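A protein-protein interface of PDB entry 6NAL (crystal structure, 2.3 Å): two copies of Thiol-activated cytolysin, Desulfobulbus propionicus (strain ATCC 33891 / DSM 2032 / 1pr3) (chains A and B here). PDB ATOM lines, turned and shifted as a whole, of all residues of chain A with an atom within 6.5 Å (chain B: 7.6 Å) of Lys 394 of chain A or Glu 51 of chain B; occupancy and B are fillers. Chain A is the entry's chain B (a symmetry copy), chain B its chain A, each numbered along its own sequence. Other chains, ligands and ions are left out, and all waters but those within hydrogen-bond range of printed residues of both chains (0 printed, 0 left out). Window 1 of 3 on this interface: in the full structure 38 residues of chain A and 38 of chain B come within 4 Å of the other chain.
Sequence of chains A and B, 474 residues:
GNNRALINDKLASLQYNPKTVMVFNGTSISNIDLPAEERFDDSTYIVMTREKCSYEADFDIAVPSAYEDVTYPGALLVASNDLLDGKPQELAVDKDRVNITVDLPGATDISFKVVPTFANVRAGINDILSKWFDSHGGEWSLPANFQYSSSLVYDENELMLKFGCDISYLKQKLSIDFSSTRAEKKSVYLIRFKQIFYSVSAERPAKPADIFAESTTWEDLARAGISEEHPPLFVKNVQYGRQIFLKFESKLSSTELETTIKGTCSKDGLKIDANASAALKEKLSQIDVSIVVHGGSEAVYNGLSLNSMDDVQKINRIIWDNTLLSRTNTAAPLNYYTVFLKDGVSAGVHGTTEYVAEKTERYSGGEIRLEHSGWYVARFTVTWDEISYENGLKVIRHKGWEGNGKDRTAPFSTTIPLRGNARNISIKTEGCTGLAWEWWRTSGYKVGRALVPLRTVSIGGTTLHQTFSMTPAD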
ATOM      1  N   ALA A  36      -2.310  -1.241   5.824  1.00  0.00           N
ATOM      2  CA  ALA A  36      -2.411  -1.594   4.415  1.00  0.00           C
ATOM      3  C   ALA A  36      -1.980  -3.044   4.220  1.00  0.00           C
ATOM      4  O   ALA A  36      -1.121  -3.581   4.933  1.00  0.00           O
ATOM      5  CB  ALA A  36      -1.564  -0.667   3.554  1.00  0.00           C
ATOM      6  N   ILE A 387       7.750  -1.081  -4.599  1.00  0.00           N
ATOM      7  CA  ILE A 387       6.984  -0.771  -3.397  1.00  0.00           C
ATOM      8  C   ILE A 387       6.581  -2.063  -2.702  1.00  0.00           C
ATOM      9  O   ILE A 387       6.290  -3.081  -3.351  1.00  0.00           O
ATOM     10  CB  ILE A 387       5.755   0.081  -3.743  1.00  0.00           C
ATOM     11  CG1 ILE A 387       6.132   1.560  -3.733  1.00  0.00           C
ATOM     12  CG2 ILE A 387       4.669  -0.057  -2.749  1.00  0.00           C
ATOM     13  CD1 ILE A 387       7.368   1.843  -4.504  1.00  0.00           C
ATOM     14  N   SER A 388       6.588  -2.015  -1.371  1.00  0.00           N
ATOM     15  CA  SER A 388       6.111  -3.079  -0.500  1.00  0.00           C
ATOM     16  C   SER A 388       5.415  -2.498   0.726  1.00  0.00           C
ATOM     17  O   SER A 388       5.753  -1.414   1.198  1.00  0.00           O
ATOM     18  CB  SER A 388       7.263  -3.951  -0.042  1.00  0.00           C
ATOM     19  OG  SER A 388       7.619  -4.870  -1.051  1.00  0.00           O
ATOM     20  N   TYR A 389       4.439  -3.228   1.245  1.00  0.00           N
ATOM     21  CA  TYR A 389       3.815  -2.900   2.532  1.00  0.00           C
ATOM     22  C   TYR A 389       4.104  -4.066   3.463  1.00  0.00           C
ATOM     23  O   TYR A 389       3.786  -5.212   3.140  1.00  0.00           O
ATOM     24  CB  TYR A 389       2.320  -2.639   2.406  1.00  0.00           C
ATOM     25  CG  TYR A 389       2.017  -1.340   1.685  1.00  0.00           C
ATOM     26  CD1 TYR A 389       1.970  -0.141   2.363  1.00  0.00           C
ATOM     27  CD2 TYR A 389       1.819  -1.320   0.318  1.00  0.00           C
ATOM     28  CE1 TYR A 389       1.699   1.051   1.695  1.00  0.00           C
ATOM     29  CE2 TYR A 389       1.553  -0.132  -0.360  1.00  0.00           C
ATOM     30  CZ  TYR A 389       1.485   1.044   0.331  1.00  0.00           C
ATOM     31  OH  TYR A 389       1.238   2.207  -0.368  1.00  0.00           O
ATOM     32  N   GLU A 390       4.826  -3.792   4.536  1.00  0.00           N
ATOM     33  CA  GLU A 390       5.217  -4.822   5.485  1.00  0.00           C
ATOM     34  C   GLU A 390       5.221  -4.170   6.860  1.00  0.00           C
ATOM     35  O   GLU A 390       5.795  -3.080   7.018  1.00  0.00           O
ATOM     36  CB  GLU A 390       6.576  -5.440   5.129  1.00  0.00           C
ATOM     37  CG  GLU A 390       7.681  -4.503   4.725  1.00  0.00           C
ATOM     38  CD  GLU A 390       8.653  -5.118   3.671  1.00  0.00           C
ATOM     39  OE1 GLU A 390       8.272  -5.269   2.475  1.00  0.00           O
ATOM     40  OE2 GLU A 390       9.823  -5.435   4.039  1.00  0.00           O
ATOM     41  N   GLY A 392       3.511  -1.864   9.337  1.00  0.00           N
ATOM     42  CA  GLY A 392       2.706  -0.740   8.885  1.00  0.00           C
ATOM     43  C   GLY A 392       3.507   0.228   8.015  1.00  0.00           C
ATOM     44  O   GLY A 392       3.258   1.441   7.940  1.00  0.00           O
ATOM     45  N   LEU A 393       4.501  -0.323   7.340  1.00  0.00           N
ATOM     46  CA  LEU A 393       5.500   0.459   6.643  1.00  0.00           C
ATOM     47  C   LEU A 393       5.321   0.367   5.132  1.00  0.00           C
ATOM     48  O   LEU A 393       5.248  -0.730   4.569  1.00  0.00           O
ATOM     49  CB  LEU A 393       6.874  -0.048   7.045  1.00  0.00           C
ATOM     50  CG  LEU A 393       7.742   0.871   7.904  1.00  0.00           C
ATOM     51  CD1 LEU A 393       9.167   0.391   7.820  1.00  0.00           C
ATOM     52  CD2 LEU A 393       7.638   2.268   7.413  1.00  0.00           C
ATOM     53  N   LYS A 394       5.258   1.510   4.480  1.00  0.00           N
ATOM     54  CA  LYS A 394       5.429   1.541   3.034  1.00  0.00           C
ATOM     55  C   LYS A 394       6.939   1.479   2.752  1.00  0.00           C
ATOM     56  O   LYS A 394       7.680   2.416   3.048  1.00  0.00           O
ATOM     57  CB  LYS A 394       4.766   2.789   2.462  1.00  0.00           C
ATOM     58  CG  LYS A 394       4.815   2.861   0.953  1.00  0.00           C
ATOM     59  CD  LYS A 394       4.372   4.253   0.471  1.00  0.00           C
ATOM     60  CE  LYS A 394       4.478   4.350  -1.052  1.00  0.00           C
ATOM     61  NZ  LYS A 394       4.282   5.753  -1.543  1.00  0.00           N
ATOM     62  N   VAL A 395       7.414   0.375   2.227  1.00  0.00           N
ATOM     63  CA  VAL A 395       8.851   0.213   1.954  1.00  0.00           C
ATOM     64  C   VAL A 395       9.121   0.456   0.475  1.00  0.00           C
ATOM     65  O   VAL A 395       8.411  -0.078  -0.388  1.00  0.00           O
ATOM     66  CB  VAL A 395       9.342  -1.182   2.374  1.00  0.00           C
ATOM     67  CG1 VAL A 395      10.767  -1.409   2.070  1.00  0.00           C
ATOM     68  CG2 VAL A 395       9.104  -1.403   3.861  1.00  0.00           C
ATOM     69  N   ILE A 396      10.167   1.240   0.185  1.00  0.00           N
ATOM     70  CA  ILE A 396      10.552   1.642  -1.175  1.00  0.00           C
ATOM     71  C   ILE A 396      11.979   1.181  -1.359  1.00  0.00           C
ATOM     72  O   ILE A 396      12.888   1.647  -0.661  1.00  0.00           O
ATOM     73  CB  ILE A 396      10.429   3.156  -1.383  1.00  0.00           C
ATOM     74  CG1 ILE A 396       8.978   3.594  -1.136  1.00  0.00           C
ATOM     75  CG2 ILE A 396      10.853   3.562  -2.783  1.00  0.00           C
ATOM     76  CD1 ILE A 396       8.832   5.095  -0.855  1.00  0.00           C
ATOM     77  N   ARG A 423       7.591   1.495  -9.620  1.00  0.00           N
ATOM     78  CA  ARG A 423       7.225   2.885  -9.832  1.00  0.00           C
ATOM     79  C   ARG A 423       8.455   3.721 -10.158  1.00  0.00           C
ATOM     80  O   ARG A 423       9.589   3.332  -9.884  1.00  0.00           O
ATOM     81  CB  ARG A 423       6.591   3.557  -8.601  1.00  0.00           C
ATOM     82  CG  ARG A 423       5.155   3.239  -8.350  1.00  0.00           C
ATOM     83  CD  ARG A 423       5.139   2.211  -7.295  1.00  0.00           C
ATOM     84  NE  ARG A 423       4.016   2.330  -6.360  1.00  0.00           N
ATOM     85  CZ  ARG A 423       2.825   1.773  -6.542  1.00  0.00           C
ATOM     86  NH1 ARG A 423       2.578   1.072  -7.656  1.00  0.00           N
ATOM     87  NH2 ARG A 423       1.888   1.933  -5.602  1.00  0.00           N
ATOM     88  N   LEU B  34      -0.634   8.940  13.497  1.00  0.00           N
ATOM     89  CA  LEU B  34      -0.563   9.886  12.384  1.00  0.00           C
ATOM     90  C   LEU B  34      -1.947  10.110  11.779  1.00  0.00           C
ATOM     91  O   LEU B  34      -2.243   9.638  10.669  1.00  0.00           O
ATOM     92  CB  LEU B  34       0.416   9.384  11.325  1.00  0.00           C
ATOM     93  CG  LEU B  34       1.901   9.311  11.666  1.00  0.00           C
ATOM     94  CD1 LEU B  34       2.684   8.798  10.389  1.00  0.00           C
ATOM     95  CD2 LEU B  34       2.464  10.609  12.116  1.00  0.00           C
ATOM     96  N   THR B  49      -2.566  14.298   5.000  1.00  0.00           N
ATOM     97  CA  THR B  49      -2.438  12.915   5.434  1.00  0.00           C
ATOM     98  C   THR B  49      -0.948  12.568   5.566  1.00  0.00           C
ATOM     99  O   THR B  49      -0.100  13.144   4.881  1.00  0.00           O
ATOM    100  CB  THR B  49      -3.172  11.992   4.447  1.00  0.00           C
ATOM    101  OG1 THR B  49      -3.192  10.661   4.975  1.00  0.00           O
ATOM    102  CG2 THR B  49      -2.534  12.010   3.055  1.00  0.00           C
ATOM    103  N   ARG B  50      -0.619  11.662   6.485  1.00  0.00           N
ATOM    104  CA  ARG B  50       0.763  11.343   6.789  1.00  0.00           C
ATOM    105  C   ARG B  50       0.943   9.846   6.744  1.00  0.00           C
ATOM    106  O   ARG B  50       0.075   9.081   7.152  1.00  0.00           O
ATOM    107  CB  ARG B  50       1.191  11.894   8.151  1.00  0.00           C
ATOM    108  CG  ARG B  50       1.400  13.414   8.122  1.00  0.00           C
ATOM    109  CD  ARG B  50       1.673  13.995   9.500  1.00  0.00           C
ATOM    110  NE  ARG B  50       0.615  13.587  10.403  1.00  0.00           N
ATOM    111  CZ  ARG B  50       0.567  13.862  11.693  1.00  0.00           C
ATOM    112  NH1 ARG B  50       1.529  14.561  12.282  1.00  0.00           N
ATOM    113  NH2 ARG B  50      -0.463  13.428  12.386  1.00  0.00           N
ATOM    114  N   GLU B  51       2.086   9.441   6.236  1.00  0.00           N
ATOM    115  CA  GLU B  51       2.387   8.035   6.062  1.00  0.00           C
ATOM    116  C   GLU B  51       3.840   7.786   6.434  1.00  0.00           C
ATOM    117  O   GLU B  51       4.736   8.551   6.064  1.00  0.00           O
ATOM    118  CB  GLU B  51       2.150   7.606   4.636  1.00  0.00           C
ATOM    119  CG  GLU B  51       1.904   6.138   4.463  1.00  0.00           C
ATOM    120  CD  GLU B  51       1.817   5.776   2.966  1.00  0.00           C
ATOM    121  OE1 GLU B  51       2.028   6.674   2.087  1.00  0.00           O
ATOM    122  OE2 GLU B  51       1.541   4.586   2.674  1.00  0.00           O
ATOM    123  N   LYS B  52       4.043   6.699   7.146  1.00  0.00           N
ATOM    124  CA  LYS B  52       5.338   6.241   7.574  1.00  0.00           C
ATOM    125  C   LYS B  52       5.900   5.383   6.458  1.00  0.00           C
ATOM    126  O   LYS B  52       5.235   4.429   6.023  1.00  0.00           O
ATOM    127  CB  LYS B  52       5.207   5.449   8.871  1.00  0.00           C
ATOM    128  CG  LYS B  52       6.545   5.015   9.454  1.00  0.00           C
ATOM    129  CD  LYS B  52       6.413   4.416  10.869  1.00  0.00           C
ATOM    130  CE  LYS B  52       7.465   3.284  11.052  1.00  0.00           C
ATOM    131  NZ  LYS B  52       8.153   3.210  12.362  1.00  0.00           N
ATOM    132  N   CYS B  53       7.118   5.733   6.001  1.00  0.00           N
ATOM    133  CA  CYS B  53       7.801   5.036   4.923  1.00  0.00           C
ATOM    134  C   CYS B  53       9.244   4.790   5.304  1.00  0.00           C
ATOM    135  O   CYS B  53       9.797   5.462   6.172  1.00  0.00           O
ATOM    136  CB  CYS B  53       7.857   5.819   3.599  1.00  0.00           C
ATOM    137  SG  CYS B  53       6.337   6.486   3.077  1.00  0.00           S
ATOM    138  N   SER B  54       9.865   3.853   4.595  1.00  0.00           N
ATOM    139  CA  SER B  54      11.294   3.643   4.641  1.00  0.00           C
ATOM    140  C   SER B  54      11.837   3.565   3.214  1.00  0.00           C
ATOM    141  O   SER B  54      11.141   3.215   2.264  1.00  0.00           O
ATOM    142  CB  SER B  54      11.630   2.413   5.458  1.00  0.00           C
ATOM    143  OG  SER B  54      11.558   1.233   4.718  1.00  0.00           O
ATOM    144  N   TYR B  55      13.055   4.017   3.055  1.00  0.00           N
ATOM    145  CA  TYR B  55      13.708   4.044   1.768  1.00  0.00           C
ATOM    146  C   TYR B  55      14.930   3.161   1.916  1.00  0.00           C
ATOM    147  O   TYR B  55      15.653   3.282   2.903  1.00  0.00           O
ATOM    148  CB  TYR B  55      14.097   5.455   1.360  1.00  0.00           C
ATOM    149  CG  TYR B  55      14.768   5.479   0.005  1.00  0.00           C
ATOM    150  CD1 TYR B  55      14.032   5.341  -1.166  1.00  0.00           C
ATOM    151  CD2 TYR B  55      16.134   5.624  -0.098  1.00  0.00           C
ATOM    152  CE1 TYR B  55      14.633   5.339  -2.408  1.00  0.00           C
ATOM    153  CE2 TYR B  55      16.788   5.624  -1.375  1.00  0.00           C
ATOM    154  CZ  TYR B  55      16.026   5.479  -2.504  1.00  0.00           C
ATOM    155  OH  TYR B  55      16.585   5.482  -3.741  1.00  0.00           O
ATOM    156  N   THR B 353      16.331   3.829   5.855  1.00  0.00           N
ATOM    157  CA  THR B 353      16.000   4.944   6.736  1.00  0.00           C
ATOM    158  C   THR B 353      14.493   5.210   6.616  1.00  0.00           C
ATOM    159  O   THR B 353      13.925   5.081   5.536  1.00  0.00           O
ATOM    160  CB  THR B 353      16.831   6.177   6.364  1.00  0.00           C
ATOM    161  OG1 THR B 353      16.623   7.225   7.331  1.00  0.00           O
ATOM    162  CG2 THR B 353      16.442   6.647   4.960  1.00  0.00           C
ATOM    163  N   GLU B 354      13.854   5.558   7.727  1.00  0.00           N
ATOM    164  CA  GLU B 354      12.428   5.808   7.756  1.00  0.00           C
ATOM    165  C   GLU B 354      12.174   7.304   7.758  1.00  0.00           C
ATOM    166  O   GLU B 354      13.026   8.104   8.137  1.00  0.00           O
ATOM    167  CB  GLU B 354      11.773   5.151   8.963  1.00  0.00           C
ATOM    168  CG  GLU B 354      12.036   3.652   8.997  1.00  0.00           C
ATOM    169  CD  GLU B 354      11.544   2.963  10.263  1.00  0.00           C
ATOM    170  OE1 GLU B 354      11.281   3.679  11.255  1.00  0.00           O
ATOM    171  OE2 GLU B 354      11.431   1.708  10.257  1.00  0.00           O
ATOM    172  N   TYR B 355      11.003   7.668   7.265  1.00  0.00           N
ATOM    173  CA  TYR B 355      10.605   9.054   7.187  1.00  0.00           C
ATOM    174  C   TYR B 355       9.084   9.113   7.178  1.00  0.00           C
ATOM    175  O   TYR B 355       8.400   8.112   6.949  1.00  0.00           O
ATOM    176  CB  TYR B 355      11.211   9.742   5.971  1.00  0.00           C
ATOM    177  CG  TYR B 355      10.846   9.175   4.630  1.00  0.00           C
ATOM    178  CD1 TYR B 355      11.549   8.127   4.078  1.00  0.00           C
ATOM    179  CD2 TYR B 355       9.855   9.762   3.877  1.00  0.00           C
ATOM    180  CE1 TYR B 355      11.232   7.643   2.796  1.00  0.00           C
ATOM    181  CE2 TYR B 355       9.535   9.306   2.621  1.00  0.00           C
ATOM    182  CZ  TYR B 355      10.223   8.232   2.089  1.00  0.00           C
ATOM    183  OH  TYR B 355       9.876   7.766   0.846  1.00  0.00           O
ATOM    184  N   VAL B 356       8.572  10.308   7.443  1.00  0.00           N
ATOM    185  CA  VAL B 356       7.146  10.604   7.393  1.00  0.00           C
ATOM    186  C   VAL B 356       6.830  11.373   6.110  1.00  0.00           C
ATOM    187  O   VAL B 356       7.200  12.542   5.970  1.00  0.00           O
ATOM    188  CB  VAL B 356       6.710  11.420   8.612  1.00  0.00           C
ATOM    189  CG1 VAL B 356       5.234  11.649   8.550  1.00  0.00           C
ATOM    190  CG2 VAL B 356       7.080  10.704   9.878  1.00  0.00           C
ATOM    191  N   ALA B 357       6.141  10.745   5.161  1.00  0.00           N
ATOM    192  CA  ALA B 357       5.738  11.447   3.940  1.00  0.00           C
ATOM    193  C   ALA B 357       4.423  12.141   4.254  1.00  0.00           C
ATOM    194  O   ALA B 357       3.499  11.493   4.767  1.00  0.00           O
ATOM    195  CB  ALA B 357       5.553  10.503   2.747  1.00  0.00           C
ATOM    196  N   GLU B 358       4.336  13.444   3.959  1.00  0.00           N
ATOM    197  CA  GLU B 358       3.107  14.219   4.155  1.00  0.00           C
ATOM    198  C   GLU B 358       2.443  14.589   2.834  1.00  0.00           C
ATOM    199  O   GLU B 358       3.055  15.232   1.987  1.00  0.00           O
ATOM    200  CB  GLU B 358       3.396  15.494   4.933  1.00  0.00           C
ATOM    201  CG  GLU B 358       4.196  15.213   6.172  1.00  0.00           C
ATOM    202  CD  GLU B 358       4.556  16.481   6.932  1.00  0.00           C
ATOM    203  OE1 GLU B 358       4.472  16.474   8.196  1.00  0.00           O
ATOM    204  OE2 GLU B 358       4.825  17.503   6.247  1.00  0.00           O
ATOM    205  N   LYS B 359       1.193  14.181   2.659  1.00  0.00           N
ATOM    206  CA  LYS B 359       0.438  14.460   1.441  1.00  0.00           C
ATOM    207  C   LYS B 359      -0.654  15.460   1.797  1.00  0.00           C
ATOM    208  O   LYS B 359      -1.432  15.231   2.718  1.00  0.00           O
ATOM    209  CB  LYS B 359      -0.173  13.199   0.827  1.00  0.00           C
ATOM    210  CG  LYS B 359      -1.043  13.529  -0.397  1.00  0.00           C
ATOM    211  CD  LYS B 359      -1.756  12.310  -0.934  1.00  0.00           C
ATOM    212  CE  LYS B 359      -2.365  12.566  -2.314  1.00  0.00           C
ATOM    213  NZ  LYS B 359      -2.056  13.909  -2.909  1.00  0.00           N
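No position is printed for both chains.
Of the 13 pairs that touch across the chains among the printed residues, none has its exchanged pair printed and touching as well.
The backbone NH (N) of Tyr 355 of chain B sits at hydrogen-bond distance from the backbone carbonyl oxygen (O) of Cys 53 of chain B (2.7 Å).
NZ of Lys 52 of chain B lies within salt-bridge range of OE1 of Glu 354 of chain B, at 3.4 Å.
The backbone NH (N) of Ala 357 of chain B is in hydrogen-bond range of the backbone carbonyl oxygen (O) of Glu 51 of chain B, 2.8 Å away.
The backbone NH (N) of Val 395 of chain A lies within hydrogen-bond range of the backbone carbonyl oxygen (O) of Ser 388 of chain A, 2.6 Å away.
The backbone NH of Tyr 55 of chain B is in hydrogen-bond range of the backbone carbonyl oxygen of Thr 353 of chain B.
The backbone NH (N) of Ser 54 of chain B sits at hydrogen-bond distance from the backbone carbonyl oxygen (O) of Lys 394 of chain A (3.0 Å).
O of Ser 54 of chain B lies within hydrogen-bond range of N of Ile 396 of chain A, at 3.0 Å.
The backbone carbonyl oxygen (O) of Lys 52 of chain B is in hydrogen-bond range of the backbone NH (N) of Lys 394 of chain A.
Of the 11 printed residues of chain A, 5 touch a printed residue of chain B.
Hydrophobic or aromatic side chains of chain A that line the printed part of chain B: Tyr 389, Leu 393, Val 395 and Ile 396.
Among the printed residues, no Asp or Glu carboxylate lies within 4 Å of a Lys or Arg side-chain nitrogen of the other chain.
Among the printed residues, merely in contact across the chains: Tyr 389 of chain A with Glu 51 of chain B, Leu 393 of chain A with Lys 52 of chain B, Leu 393 of chain A with Cys 53 of chain B, Leu 393 of chain A with Ser 54 of chain B, Leu 393 of chain A with Glu 354 of chain B, Lys 394 of chain A with Glu 51 of chain B, Lys 394 of chain A with Cys 53 of chain B, Val 395 of chain A with Ser 54 of chain B, Ile 396 of chain A with Tyr 55 of chain B and Ile 396 of chain A with Tyr 355 of chain B.
Of the printed residues of chain B, Tyr 389 of chain A touches Glu 51.
Of chain B, only Glu 51 (3.6 Å), Lys 52 (3.3 Å), Cys 53 (3.2 Å) and Ser 54 (3.0 Å) come within 4 Å of Lys 394 of chain A.
Printed residues of chain B within 4 Å of Ile 396 of chain A: Ser 54 (3.0 Å), Tyr 55 (3.5 Å) and Tyr 355 (3.3 Å).
Arg 423 of chain A touches none of the printed residues of chain B.
Of chain A, only Tyr 389 (3.7 Å) and Lys 394 (3.6 Å) come within 4 Å of Glu 51 of chain B.
Of the printed residues of chain A, Lys 52 of chain B touches Leu 393 (3.5 Å) and Lys 394 (3.3 Å).
Of the printed residues of chain A, Glu 354 of chain B touches Leu 393.
Printed residues of chain A within 4 Å of Tyr 355 of chain B: Ile 396.
The nearest residue of chain B that does not touch Lys 394 of chain A is Tyr 55 of chain B (5.6 Å).
The nearest residue of chain A that does not touch Glu 51 of chain B is Gly 392 of chain A (6.0 Å).
The nearest printed residue of chain A that does not touch Tyr 55 of chain B is Lys 394 of chain A (5.6 Å).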
